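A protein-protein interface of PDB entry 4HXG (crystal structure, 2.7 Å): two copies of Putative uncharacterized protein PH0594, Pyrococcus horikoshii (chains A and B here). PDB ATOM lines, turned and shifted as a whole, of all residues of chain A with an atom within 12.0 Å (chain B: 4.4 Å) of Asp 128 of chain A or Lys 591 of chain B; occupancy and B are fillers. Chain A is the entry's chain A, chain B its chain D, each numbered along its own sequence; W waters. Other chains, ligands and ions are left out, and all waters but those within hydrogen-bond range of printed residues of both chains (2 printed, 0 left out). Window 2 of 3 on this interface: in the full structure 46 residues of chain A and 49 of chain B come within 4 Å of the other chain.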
ATOM      1  N   ASN A 105      -8.938   5.998  -7.476  1.00  0.00           N
ATOM      2  CA  ASN A 105      -7.542   6.123  -7.062  1.00  0.00           C
ATOM      3  C   ASN A 105      -7.308   6.285  -5.567  1.00  0.00           C
ATOM      4  O   ASN A 105      -6.572   7.177  -5.144  1.00  0.00           O
ATOM      5  CB  ASN A 105      -6.887   7.294  -7.791  1.00  0.00           C
ATOM      6  CG  ASN A 105      -7.048   7.204  -9.286  1.00  0.00           C
ATOM      7  OD1 ASN A 105      -7.280   6.123  -9.830  1.00  0.00           O
ATOM      8  ND2 ASN A 105      -6.922   8.338  -9.965  1.00  0.00           N
ATOM      9  N   PHE A 123      -3.965   8.823  -5.351  1.00  0.00           N
ATOM     10  CA  PHE A 123      -3.130   9.524  -6.320  1.00  0.00           C
ATOM     11  C   PHE A 123      -3.918  10.380  -7.313  1.00  0.00           C
ATOM     12  O   PHE A 123      -5.140  10.277  -7.406  1.00  0.00           O
ATOM     13  CB  PHE A 123      -2.227   8.542  -7.058  1.00  0.00           C
ATOM     14  CG  PHE A 123      -2.965   7.431  -7.734  1.00  0.00           C
ATOM     15  CD1 PHE A 123      -3.380   6.323  -7.016  1.00  0.00           C
ATOM     16  CD2 PHE A 123      -3.234   7.486  -9.093  1.00  0.00           C
ATOM     17  CE1 PHE A 123      -4.057   5.282  -7.643  1.00  0.00           C
ATOM     18  CE2 PHE A 123      -3.908   6.454  -9.729  1.00  0.00           C
ATOM     19  CZ  PHE A 123      -4.322   5.350  -9.003  1.00  0.00           C
ATOM     20  N   LYS A 124      -3.206  11.254  -8.021  1.00  0.00           N
ATOM     21  CA  LYS A 124      -3.790  12.062  -9.085  1.00  0.00           C
ATOM     22  C   LYS A 124      -2.803  12.159 -10.237  1.00  0.00           C
ATOM     23  O   LYS A 124      -1.634  12.461 -10.022  1.00  0.00           O
ATOM     24  CB  LYS A 124      -4.133  13.467  -8.578  1.00  0.00           C
ATOM     25  N   ARG A 125      -3.276  11.919 -11.458  1.00  0.00           N
ATOM     26  CA  ARG A 125      -2.413  11.999 -12.634  1.00  0.00           C
ATOM     27  C   ARG A 125      -2.919  13.028 -13.614  1.00  0.00           C
ATOM     28  O   ARG A 125      -3.978  13.616 -13.408  1.00  0.00           O
ATOM     29  CB  ARG A 125      -2.363  10.654 -13.336  1.00  0.00           C
ATOM     30  CG  ARG A 125      -1.958   9.553 -12.421  1.00  0.00           C
ATOM     31  CD  ARG A 125      -1.788   8.265 -13.157  1.00  0.00           C
ATOM     32  NE  ARG A 125      -1.162   7.295 -12.279  1.00  0.00           N
ATOM     33  CZ  ARG A 125      -1.209   5.987 -12.470  1.00  0.00           C
ATOM     34  NH1 ARG A 125      -1.856   5.486 -13.520  1.00  0.00           N
ATOM     35  NH2 ARG A 125      -0.609   5.182 -11.607  1.00  0.00           N
ATOM     36  N   ARG A 126      -2.177  13.221 -14.700  1.00  0.00           N
ATOM     37  CA  ARG A 126      -2.579  14.175 -15.728  1.00  0.00           C
ATOM     38  C   ARG A 126      -3.849  13.735 -16.482  1.00  0.00           C
ATOM     39  O   ARG A 126      -4.705  14.562 -16.788  1.00  0.00           O
ATOM     40  CB  ARG A 126      -1.415  14.462 -16.679  1.00  0.00           C
ATOM     41  CG  ARG A 126      -0.392  15.409 -16.077  1.00  0.00           C
ATOM     42  CD  ARG A 126       0.863  15.544 -16.930  1.00  0.00           C
ATOM     43  NE  ARG A 126       1.797  16.511 -16.355  1.00  0.00           N
ATOM     44  CZ  ARG A 126       2.955  16.191 -15.778  1.00  0.00           C
ATOM     45  NH1 ARG A 126       3.738  17.140 -15.276  1.00  0.00           N
ATOM     46  NH2 ARG A 126       3.343  14.923 -15.708  1.00  0.00           N
ATOM     47  N   GLU A 127      -3.958  12.436 -16.765  1.00  0.00           N
ATOM     48  CA  GLU A 127      -5.175  11.814 -17.311  1.00  0.00           C
ATOM     49  C   GLU A 127      -5.629  12.233 -18.722  1.00  0.00           C
ATOM     50  O   GLU A 127      -6.818  12.143 -19.035  1.00  0.00           O
ATOM     51  CB  GLU A 127      -6.348  11.961 -16.329  1.00  0.00           C
ATOM     52  CG  GLU A 127      -6.085  11.454 -14.913  1.00  0.00           C
ATOM     53  CD  GLU A 127      -5.915   9.943 -14.829  1.00  0.00           C
ATOM     54  OE1 GLU A 127      -5.504   9.328 -15.837  1.00  0.00           O
ATOM     55  OE2 GLU A 127      -6.194   9.370 -13.749  1.00  0.00           O
ATOM     56  N   ASP A 128      -4.709  12.668 -19.577  1.00  0.00           N
ATOM     57  CA  ASP A 128      -5.092  12.963 -20.956  1.00  0.00           C
ATOM     58  C   ASP A 128      -5.411  11.676 -21.711  1.00  0.00           C
ATOM     59  O   ASP A 128      -4.679  10.697 -21.627  1.00  0.00           O
ATOM     60  CB  ASP A 128      -4.004  13.740 -21.694  1.00  0.00           C
ATOM     61  CG  ASP A 128      -4.364  14.000 -23.149  1.00  0.00           C
ATOM     62  OD1 ASP A 128      -4.915  15.081 -23.445  1.00  0.00           O
ATOM     63  OD2 ASP A 128      -4.106  13.119 -23.997  1.00  0.00           O
ATOM     64  N   GLU A 129      -6.505  11.688 -22.461  1.00  0.00           N
ATOM     65  CA  GLU A 129      -6.986  10.486 -23.133  1.00  0.00           C
ATOM     66  C   GLU A 129      -5.972   9.930 -24.127  1.00  0.00           C
ATOM     67  O   GLU A 129      -5.788   8.721 -24.212  1.00  0.00           O
ATOM     68  CB  GLU A 129      -8.328  10.745 -23.824  1.00  0.00           C
ATOM     69  N   ASP A 130      -5.340  10.805 -24.901  1.00  0.00           N
ATOM     70  CA  ASP A 130      -4.412  10.401 -25.962  1.00  0.00           C
ATOM     71  C   ASP A 130      -2.967  10.068 -25.584  1.00  0.00           C
ATOM     72  O   ASP A 130      -2.344   9.196 -26.192  1.00  0.00           O
ATOM     73  CB  ASP A 130      -4.450  11.416 -27.079  1.00  0.00           C
ATOM     74  CG  ASP A 130      -5.838  11.658 -27.552  1.00  0.00           C
ATOM     75  OD1 ASP A 130      -6.570  10.662 -27.719  1.00  0.00           O
ATOM     76  OD2 ASP A 130      -6.203  12.839 -27.714  1.00  0.00           O
ATOM     77  N   PHE A 131      -2.410  10.811 -24.639  1.00  0.00           N
ATOM     78  CA  PHE A 131      -1.003  10.630 -24.352  1.00  0.00           C
ATOM     79  C   PHE A 131      -0.642  10.868 -22.898  1.00  0.00           C
ATOM     80  O   PHE A 131      -1.345  11.570 -22.160  1.00  0.00           O
ATOM     81  CB  PHE A 131      -0.143  11.506 -25.265  1.00  0.00           C
ATOM     82  CG  PHE A 131      -0.118  12.949 -24.861  1.00  0.00           C
ATOM     83  CD1 PHE A 131      -1.014  13.853 -25.409  1.00  0.00           C
ATOM     84  CD2 PHE A 131       0.795  13.401 -23.932  1.00  0.00           C
ATOM     85  CE1 PHE A 131      -1.000  15.176 -25.043  1.00  0.00           C
ATOM     86  CE2 PHE A 131       0.812  14.727 -23.558  1.00  0.00           C
ATOM     87  CZ  PHE A 131      -0.088  15.617 -24.116  1.00  0.00           C
ATOM     88  N   ILE A 132       0.470  10.251 -22.513  1.00  0.00           N
ATOM     89  CA  ILE A 132       1.044  10.337 -21.188  1.00  0.00           C
ATOM     90  C   ILE A 132       2.229  11.274 -21.308  1.00  0.00           C
ATOM     91  O   ILE A 132       2.928  11.256 -22.317  1.00  0.00           O
ATOM     92  CB  ILE A 132       1.555   8.956 -20.776  1.00  0.00           C
ATOM     93  CG1 ILE A 132       0.379   8.042 -20.444  1.00  0.00           C
ATOM     94  CG2 ILE A 132       2.508   9.047 -19.608  1.00  0.00           C
ATOM     95  CD1 ILE A 132       0.664   6.597 -20.743  1.00  0.00           C
ATOM     96  N   PHE A 133       2.455  12.101 -20.296  1.00  0.00           N
ATOM     97  CA  PHE A 133       3.563  13.033 -20.337  1.00  0.00           C
ATOM     98  C   PHE A 133       4.353  12.954 -19.046  1.00  0.00           C
ATOM     99  O   PHE A 133       3.794  13.119 -17.966  1.00  0.00           O
ATOM    100  CB  PHE A 133       3.046  14.448 -20.533  1.00  0.00           C
ATOM    101  CG  PHE A 133       4.124  15.445 -20.789  1.00  0.00           C
ATOM    102  CD1 PHE A 133       4.761  15.494 -22.022  1.00  0.00           C
ATOM    103  CD2 PHE A 133       4.502  16.344 -19.801  1.00  0.00           C
ATOM    104  CE1 PHE A 133       5.755  16.427 -22.263  1.00  0.00           C
ATOM    105  CE2 PHE A 133       5.497  17.276 -20.032  1.00  0.00           C
ATOM    106  CZ  PHE A 133       6.124  17.321 -21.265  1.00  0.00           C
ATOM    107  N   GLU A 134       5.655  12.715 -19.153  1.00  0.00           N
ATOM    108  CA  GLU A 134       6.455  12.482 -17.959  1.00  0.00           C
ATOM    109  C   GLU A 134       7.667  13.388 -17.871  1.00  0.00           C
ATOM    110  O   GLU A 134       8.524  13.366 -18.756  1.00  0.00           O
ATOM    111  CB  GLU A 134       6.902  11.026 -17.901  1.00  0.00           C
ATOM    112  CG  GLU A 134       7.620  10.674 -16.616  1.00  0.00           C
ATOM    113  CD  GLU A 134       6.761  10.918 -15.400  1.00  0.00           C
ATOM    114  OE1 GLU A 134       7.131  11.791 -14.592  1.00  0.00           O
ATOM    115  OE2 GLU A 134       5.722  10.238 -15.250  1.00  0.00           O
ATOM    116  N   PHE A 146       1.456   3.512 -16.106  1.00  0.00           N
ATOM    117  CA  PHE A 146       2.197   4.748 -16.374  1.00  0.00           C
ATOM    118  C   PHE A 146       1.864   5.825 -15.343  1.00  0.00           C
ATOM    119  O   PHE A 146       0.693   6.090 -15.080  1.00  0.00           O
ATOM    120  CB  PHE A 146       1.891   5.277 -17.782  1.00  0.00           C
ATOM    121  CG  PHE A 146       2.603   4.541 -18.884  1.00  0.00           C
ATOM    122  CD1 PHE A 146       1.994   3.478 -19.544  1.00  0.00           C
ATOM    123  CD2 PHE A 146       3.881   4.919 -19.272  1.00  0.00           C
ATOM    124  CE1 PHE A 146       2.647   2.802 -20.564  1.00  0.00           C
ATOM    125  CE2 PHE A 146       4.543   4.244 -20.293  1.00  0.00           C
ATOM    126  CZ  PHE A 146       3.921   3.184 -20.939  1.00  0.00           C
ATOM    127  N   PHE A 147       2.892   6.451 -14.773  1.00  0.00           N
ATOM    128  CA  PHE A 147       2.688   7.443 -13.721  1.00  0.00           C
ATOM    129  C   PHE A 147       1.965   8.682 -14.254  1.00  0.00           C
ATOM    130  O   PHE A 147       1.132   9.259 -13.562  1.00  0.00           O
ATOM    131  CB  PHE A 147       4.023   7.838 -13.061  1.00  0.00           C
ATOM    132  CG  PHE A 147       4.417   6.975 -11.873  1.00  0.00           C
ATOM    133  CD1 PHE A 147       5.694   6.425 -11.790  1.00  0.00           C
ATOM    134  CD2 PHE A 147       3.530   6.739 -10.834  1.00  0.00           C
ATOM    135  CE1 PHE A 147       6.077   5.639 -10.706  1.00  0.00           C
ATOM    136  CE2 PHE A 147       3.908   5.951  -9.741  1.00  0.00           C
ATOM    137  CZ  PHE A 147       5.188   5.403  -9.682  1.00  0.00           C
ATOM    138  N   ASP A 148       2.280   9.086 -15.480  1.00  0.00           N
ATOM    139  CA  ASP A 148       1.649  10.257 -16.083  1.00  0.00           C
ATOM    140  C   ASP A 148       1.638  11.431 -15.107  1.00  0.00           C
ATOM    141  O   ASP A 148       0.603  12.069 -14.902  1.00  0.00           O
ATOM    142  CB  ASP A 148       0.226   9.932 -16.550  1.00  0.00           C
ATOM    143  CG  ASP A 148      -0.321  10.961 -17.536  1.00  0.00           C
ATOM    144  OD1 ASP A 148       0.483  11.611 -18.235  1.00  0.00           O
ATOM    145  OD2 ASP A 148      -1.559  11.114 -17.621  1.00  0.00           O
ATOM    146  N   GLY A 149       2.795  11.704 -14.504  1.00  0.00           N
ATOM    147  CA  GLY A 149       2.953  12.831 -13.597  1.00  0.00           C
ATOM    148  C   GLY A 149       2.283  12.675 -12.242  1.00  0.00           C
ATOM    149  O   GLY A 149       1.930  13.664 -11.593  1.00  0.00           O
ATOM    150  N   GLU A 150       2.122  11.429 -11.807  1.00  0.00           N
ATOM    151  CA  GLU A 150       1.423  11.125 -10.563  1.00  0.00           C
ATOM    152  C   GLU A 150       1.959  11.890  -9.353  1.00  0.00           C
ATOM    153  O   GLU A 150       3.165  12.083  -9.194  1.00  0.00           O
ATOM    154  CB  GLU A 150       1.461   9.618 -10.287  1.00  0.00           C
ATOM    155  CG  GLU A 150       0.884   9.214  -8.939  1.00  0.00           C
ATOM    156  CD  GLU A 150       0.771   7.714  -8.791  1.00  0.00           C
ATOM    157  OE1 GLU A 150       0.538   7.046  -9.821  1.00  0.00           O
ATOM    158  OE2 GLU A 150       0.923   7.202  -7.657  1.00  0.00           O
ATOM    159  N   LYS B 574      -0.778   6.825 -26.305  1.00  0.00           N
ATOM    160  CA  LYS B 574      -1.344   5.544 -25.919  1.00  0.00           C
ATOM    161  C   LYS B 574      -1.699   4.676 -27.127  1.00  0.00           C
ATOM    162  O   LYS B 574      -1.789   3.456 -27.019  1.00  0.00           O
ATOM    163  CB  LYS B 574      -2.571   5.757 -25.032  1.00  0.00           C
ATOM    164  CG  LYS B 574      -2.298   6.571 -23.775  1.00  0.00           C
ATOM    165  CD  LYS B 574      -3.033   5.995 -22.578  1.00  0.00           C
ATOM    166  CE  LYS B 574      -4.232   6.841 -22.195  1.00  0.00           C
ATOM    167  NZ  LYS B 574      -3.824   7.996 -21.354  1.00  0.00           N
ATOM    168  N   ARG B 587      -7.657  13.620 -33.369  1.00  0.00           N
ATOM    169  CA  ARG B 587      -7.491  14.305 -32.095  1.00  0.00           C
ATOM    170  C   ARG B 587      -6.081  14.080 -31.545  1.00  0.00           C
ATOM    171  O   ARG B 587      -5.447  14.998 -31.038  1.00  0.00           O
ATOM    172  CB  ARG B 587      -8.550  13.867 -31.087  1.00  0.00           C
ATOM    173  CG  ARG B 587      -8.614  14.784 -29.881  1.00  0.00           C
ATOM    174  CD  ARG B 587      -9.488  14.205 -28.803  1.00  0.00           C
ATOM    175  NE  ARG B 587      -9.007  12.898 -28.374  1.00  0.00           N
ATOM    176  CZ  ARG B 587      -9.798  11.877 -28.064  1.00  0.00           C
ATOM    177  NH1 ARG B 587     -11.114  12.015 -28.140  1.00  0.00           N
ATOM    178  NH2 ARG B 587      -9.277  10.723 -27.682  1.00  0.00           N
ATOM    179  N   HIS B 588      -5.609  12.844 -31.670  1.00  0.00           N
ATOM    180  CA  HIS B 588      -4.253  12.446 -31.308  1.00  0.00           C
ATOM    181  C   HIS B 588      -3.256  13.320 -32.059  1.00  0.00           C
ATOM    182  O   HIS B 588      -2.410  13.980 -31.450  1.00  0.00           O
ATOM    183  CB  HIS B 588      -4.080  10.954 -31.653  1.00  0.00           C
ATOM    184  CG  HIS B 588      -2.668  10.451 -31.607  1.00  0.00           C
ATOM    185  ND1 HIS B 588      -2.346   9.213 -31.092  1.00  0.00           N
ATOM    186  CD2 HIS B 588      -1.506  10.984 -32.055  1.00  0.00           C
ATOM    187  CE1 HIS B 588      -1.045   9.019 -31.197  1.00  0.00           C
ATOM    188  NE2 HIS B 588      -0.511  10.076 -31.780  1.00  0.00           N
ATOM    189  N   ARG B 589      -3.377  13.336 -33.385  1.00  0.00           N
ATOM    190  CA  ARG B 589      -2.465  14.098 -34.231  1.00  0.00           C
ATOM    191  C   ARG B 589      -2.487  15.582 -33.888  1.00  0.00           C
ATOM    192  O   ARG B 589      -1.461  16.256 -33.947  1.00  0.00           O
ATOM    193  CB  ARG B 589      -2.792  13.891 -35.707  1.00  0.00           C
ATOM    194  CG  ARG B 589      -2.537  12.488 -36.221  1.00  0.00           C
ATOM    195  CD  ARG B 589      -2.857  12.399 -37.702  1.00  0.00           C
ATOM    196  NE  ARG B 589      -2.062  13.348 -38.482  1.00  0.00           N
ATOM    197  CZ  ARG B 589      -2.410  13.832 -39.672  1.00  0.00           C
ATOM    198  NH1 ARG B 589      -3.555  13.470 -40.236  1.00  0.00           N
ATOM    199  NH2 ARG B 589      -1.613  14.687 -40.295  1.00  0.00           N
ATOM    200  N   MET B 590      -3.657  16.095 -33.530  1.00  0.00           N
ATOM    201  CA  MET B 590      -3.750  17.496 -33.157  1.00  0.00           C
ATOM    202  C   MET B 590      -2.922  17.760 -31.915  1.00  0.00           C
ATOM    203  O   MET B 590      -2.083  18.663 -31.894  1.00  0.00           O
ATOM    204  CB  MET B 590      -5.190  17.901 -32.889  1.00  0.00           C
ATOM    205  CG  MET B 590      -5.306  19.296 -32.317  1.00  0.00           C
ATOM    206  SD  MET B 590      -6.717  19.410 -31.233  1.00  0.00           S
ATOM    207  CE  MET B 590      -6.154  18.461 -29.835  1.00  0.00           C
ATOM    208  N   LYS B 591      -3.161  16.973 -30.875  1.00  0.00           N
ATOM    209  CA  LYS B 591      -2.374  17.103 -29.665  1.00  0.00           C
ATOM    210  C   LYS B 591      -0.887  17.025 -29.960  1.00  0.00           C
ATOM    211  O   LYS B 591      -0.114  17.825 -29.430  1.00  0.00           O
ATOM    212  CB  LYS B 591      -2.789  16.064 -28.643  1.00  0.00           C
ATOM    213  CG  LYS B 591      -4.131  16.399 -28.077  1.00  0.00           C
ATOM    214  CD  LYS B 591      -4.648  15.340 -27.173  1.00  0.00           C
ATOM    215  CE  LYS B 591      -5.995  15.758 -26.655  1.00  0.00           C
ATOM    216  NZ  LYS B 591      -6.538  14.733 -25.745  1.00  0.00           N
ATOM    217  N   ARG B 592      -0.478  16.094 -30.820  1.00  0.00           N
ATOM    218  CA  ARG B 592       0.933  16.034 -31.166  1.00  0.00           C
ATOM    219  C   ARG B 592       1.427  17.333 -31.784  1.00  0.00           C
ATOM    220  O   ARG B 592       2.498  17.817 -31.427  1.00  0.00           O
ATOM    221  CB  ARG B 592       1.274  14.878 -32.094  1.00  0.00           C
ATOM    222  CG  ARG B 592       2.756  14.909 -32.450  1.00  0.00           C
ATOM    223  CD  ARG B 592       3.174  13.773 -33.348  1.00  0.00           C
ATOM    224  NE  ARG B 592       4.395  14.102 -34.075  1.00  0.00           N
ATOM    225  CZ  ARG B 592       4.453  15.004 -35.048  1.00  0.00           C
ATOM    226  NH1 ARG B 592       5.603  15.248 -35.665  1.00  0.00           N
ATOM    227  NH2 ARG B 592       3.361  15.670 -35.402  1.00  0.00           N
ATOM    228  N   TYR B 593       0.659  17.894 -32.715  1.00  0.00           N
ATOM    229  CA  TYR B 593       1.062  19.139 -33.365  1.00  0.00           C
ATOM    230  C   TYR B 593       1.182  20.275 -32.358  1.00  0.00           C
ATOM    231  O   TYR B 593       2.186  20.989 -32.319  1.00  0.00           O
ATOM    232  CB  TYR B 593       0.079  19.519 -34.469  1.00  0.00           C
ATOM    233  CG  TYR B 593       0.170  18.634 -35.686  1.00  0.00           C
ATOM    234  CD1 TYR B 593      -0.966  18.072 -36.239  1.00  0.00           C
ATOM    235  CD2 TYR B 593       1.390  18.367 -36.285  1.00  0.00           C
ATOM    236  CE1 TYR B 593      -0.894  17.263 -37.349  1.00  0.00           C
ATOM    237  CE2 TYR B 593       1.475  17.560 -37.397  1.00  0.00           C
ATOM    238  CZ  TYR B 593       0.329  17.012 -37.926  1.00  0.00           C
ATOM    239  OH  TYR B 593       0.399  16.203 -39.036  1.00  0.00           O
ATOM    240  N   LYS B 594       0.154  20.432 -31.535  1.00  0.00           N
ATOM    241  CA  LYS B 594       0.145  21.498 -30.549  1.00  0.00           C
ATOM    242  C   LYS B 594       1.382  21.382 -29.664  1.00  0.00           C
ATOM    243  O   LYS B 594       2.001  22.380 -29.311  1.00  0.00           O
ATOM    244  CB  LYS B 594      -1.151  21.453 -29.729  1.00  0.00           C
ATOM    245  CG  LYS B 594      -1.286  22.524 -28.660  1.00  0.00           C
ATOM    246  CD  LYS B 594      -1.269  23.921 -29.255  1.00  0.00           C
ATOM    247  CE  LYS B 594      -1.313  24.984 -28.161  1.00  0.00           C
ATOM    248  NZ  LYS B 594      -1.481  26.370 -28.697  1.00  0.00           N
ATOM    249  N   LEU B 595       1.750  20.150 -29.336  1.00  0.00           N
ATOM    250  CA  LEU B 595       2.898  19.872 -28.481  1.00  0.00           C
ATOM    251  C   LEU B 595       4.216  20.263 -29.157  1.00  0.00           C
ATOM    252  O   LEU B 595       5.034  20.987 -28.585  1.00  0.00           O
ATOM    253  CB  LEU B 595       2.912  18.386 -28.114  1.00  0.00           C
ATOM    254  CG  LEU B 595       3.796  17.958 -26.944  1.00  0.00           C
ATOM    255  CD1 LEU B 595       3.377  18.705 -25.694  1.00  0.00           C
ATOM    256  CD2 LEU B 595       3.703  16.459 -26.733  1.00  0.00           C
ATOM    257  N   LEU B 617      -1.413  22.925 -23.256  1.00  0.00           N
ATOM    258  CA  LEU B 617      -2.440  22.444 -24.182  1.00  0.00           C
ATOM    259  C   LEU B 617      -3.814  22.658 -23.541  1.00  0.00           C
ATOM    260  O   LEU B 617      -4.179  21.968 -22.589  1.00  0.00           O
ATOM    261  CB  LEU B 617      -2.250  20.952 -24.508  1.00  0.00           C
ATOM    262  CG  LEU B 617      -0.919  20.367 -25.010  1.00  0.00           C
ATOM    263  CD1 LEU B 617      -1.163  19.482 -26.226  1.00  0.00           C
ATOM    264  CD2 LEU B 617       0.129  21.427 -25.324  1.00  0.00           C
HETATM  265  O   HOH W   1      -2.949   7.888 -28.658  1.00  0.00           O
HETATM  266  O   HOH W   2      -3.353   9.671 -19.371  1.00  0.00           O
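Asp 128 of chain A touches just these residues of chain B: Lys 574 and Lys 591.
Of the printed residues of chain B, Asp 130 of chain A touches Lys 574, Arg 587 and Lys 591.
Glu 134 of chain A touches none of the printed residues of chain B.
Of the printed residues of chain A, Lys 574 of chain B touches Asp 128 (2.8 Å), Glu 129 (3.2 Å) and Asp 130 (2.8 Å).
Of chain A, only Glu 129 (3.97 Å) and Asp 130 (2.7 Å) come within 4 Å of Arg 587 of chain B.
No residue of chain A comes within 4 Å of Met 590 of chain B.
Of chain A, only Asp 128 and Asp 130 come within 4 Å of Lys 591 of chain B.
Lys 594 of chain B touches none of the printed residues of chain A.
Leu 595 of chain B touches none of the printed residues of chain A.
The nearest residue of chain A that does not touch Lys 591 of chain B is Phe 131 of chain A (4.1 Å).
The nearest printed residue of chain A that does not touch Lys 574 of chain B is Ile 132 of chain A (4.2 Å).
OD2 of Asp 128 of chain A is in hydrogen-bond range of N of Phe 131 of chain A (2.9 Å).
The backbone NH of Asp 130 of chain A is in hydrogen-bond range of the side-chain carboxylate of Asp 128 of chain A (2.8 Å).
OD1 of Asp 130 of chain A lies within salt-bridge range of NH2 of Arg 587 of chain B (2.7 Å).
OD1 of Asp 128 of chain A lies within salt-bridge range of NZ of Lys 591 of chain B, 2.8 Å away.
The side-chain carboxylate of Asp 130 of chain A lies within salt-bridge range of the side-chain amino group of Lys 591 of chain B (2.8 Å).
The backbone carbonyl oxygen (O) of Asp 128 of chain A sits at hydrogen-bond distance from the side-chain amino group (NZ) of Lys 574 of chain B, at 2.8 Å.
The backbone NH (N) of Lys 574 of chain B lies within hydrogen-bond range of the backbone carbonyl oxygen (O) of Asp 130 of chain A, 2.8 Å away.
No position is printed for both chains.
Of the 7 pairs that touch across the chains among the printed residues, none has its exchanged pair printed and touching as well.
Water W2 lies within hydrogen-bond range of the side-chain amino group (NZ) of Lys 574 of chain B (2.6 Å), the backbone carbonyl oxygen (O) of Asp 128 of chain A (2.8 Å) and the side-chain carboxylate (OD2) of Asp 148 of chain A (2.9 Å).
Water W1 lies within hydrogen-bond range of a ring nitrogen (ND1) of His 588 of chain B (2.8 Å), the backbone carbonyl oxygen of Asp 130 of chain A (2.9 Å) and the backbone NH of Lys 574 of chain B (3.4 Å).
Among the printed residues, 7 pairs touch across the chains.
Among the printed residues, Asp or Glu carboxylates within 4 Å of a Lys or Arg side-chain nitrogen of the other chain: Asp 128 of chain A with Lys 591 of chain B, Asp 130 of chain A with Arg 587 of chain B and Asp 130 of chain A with Lys 591 of chain B.
Among the printed residues, merely in contact across the chains: Glu 129 of chain A with Lys 574 of chain B (3.2 Å) and Glu 129 of chain A with Arg 587 of chain B (3.97 Å).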
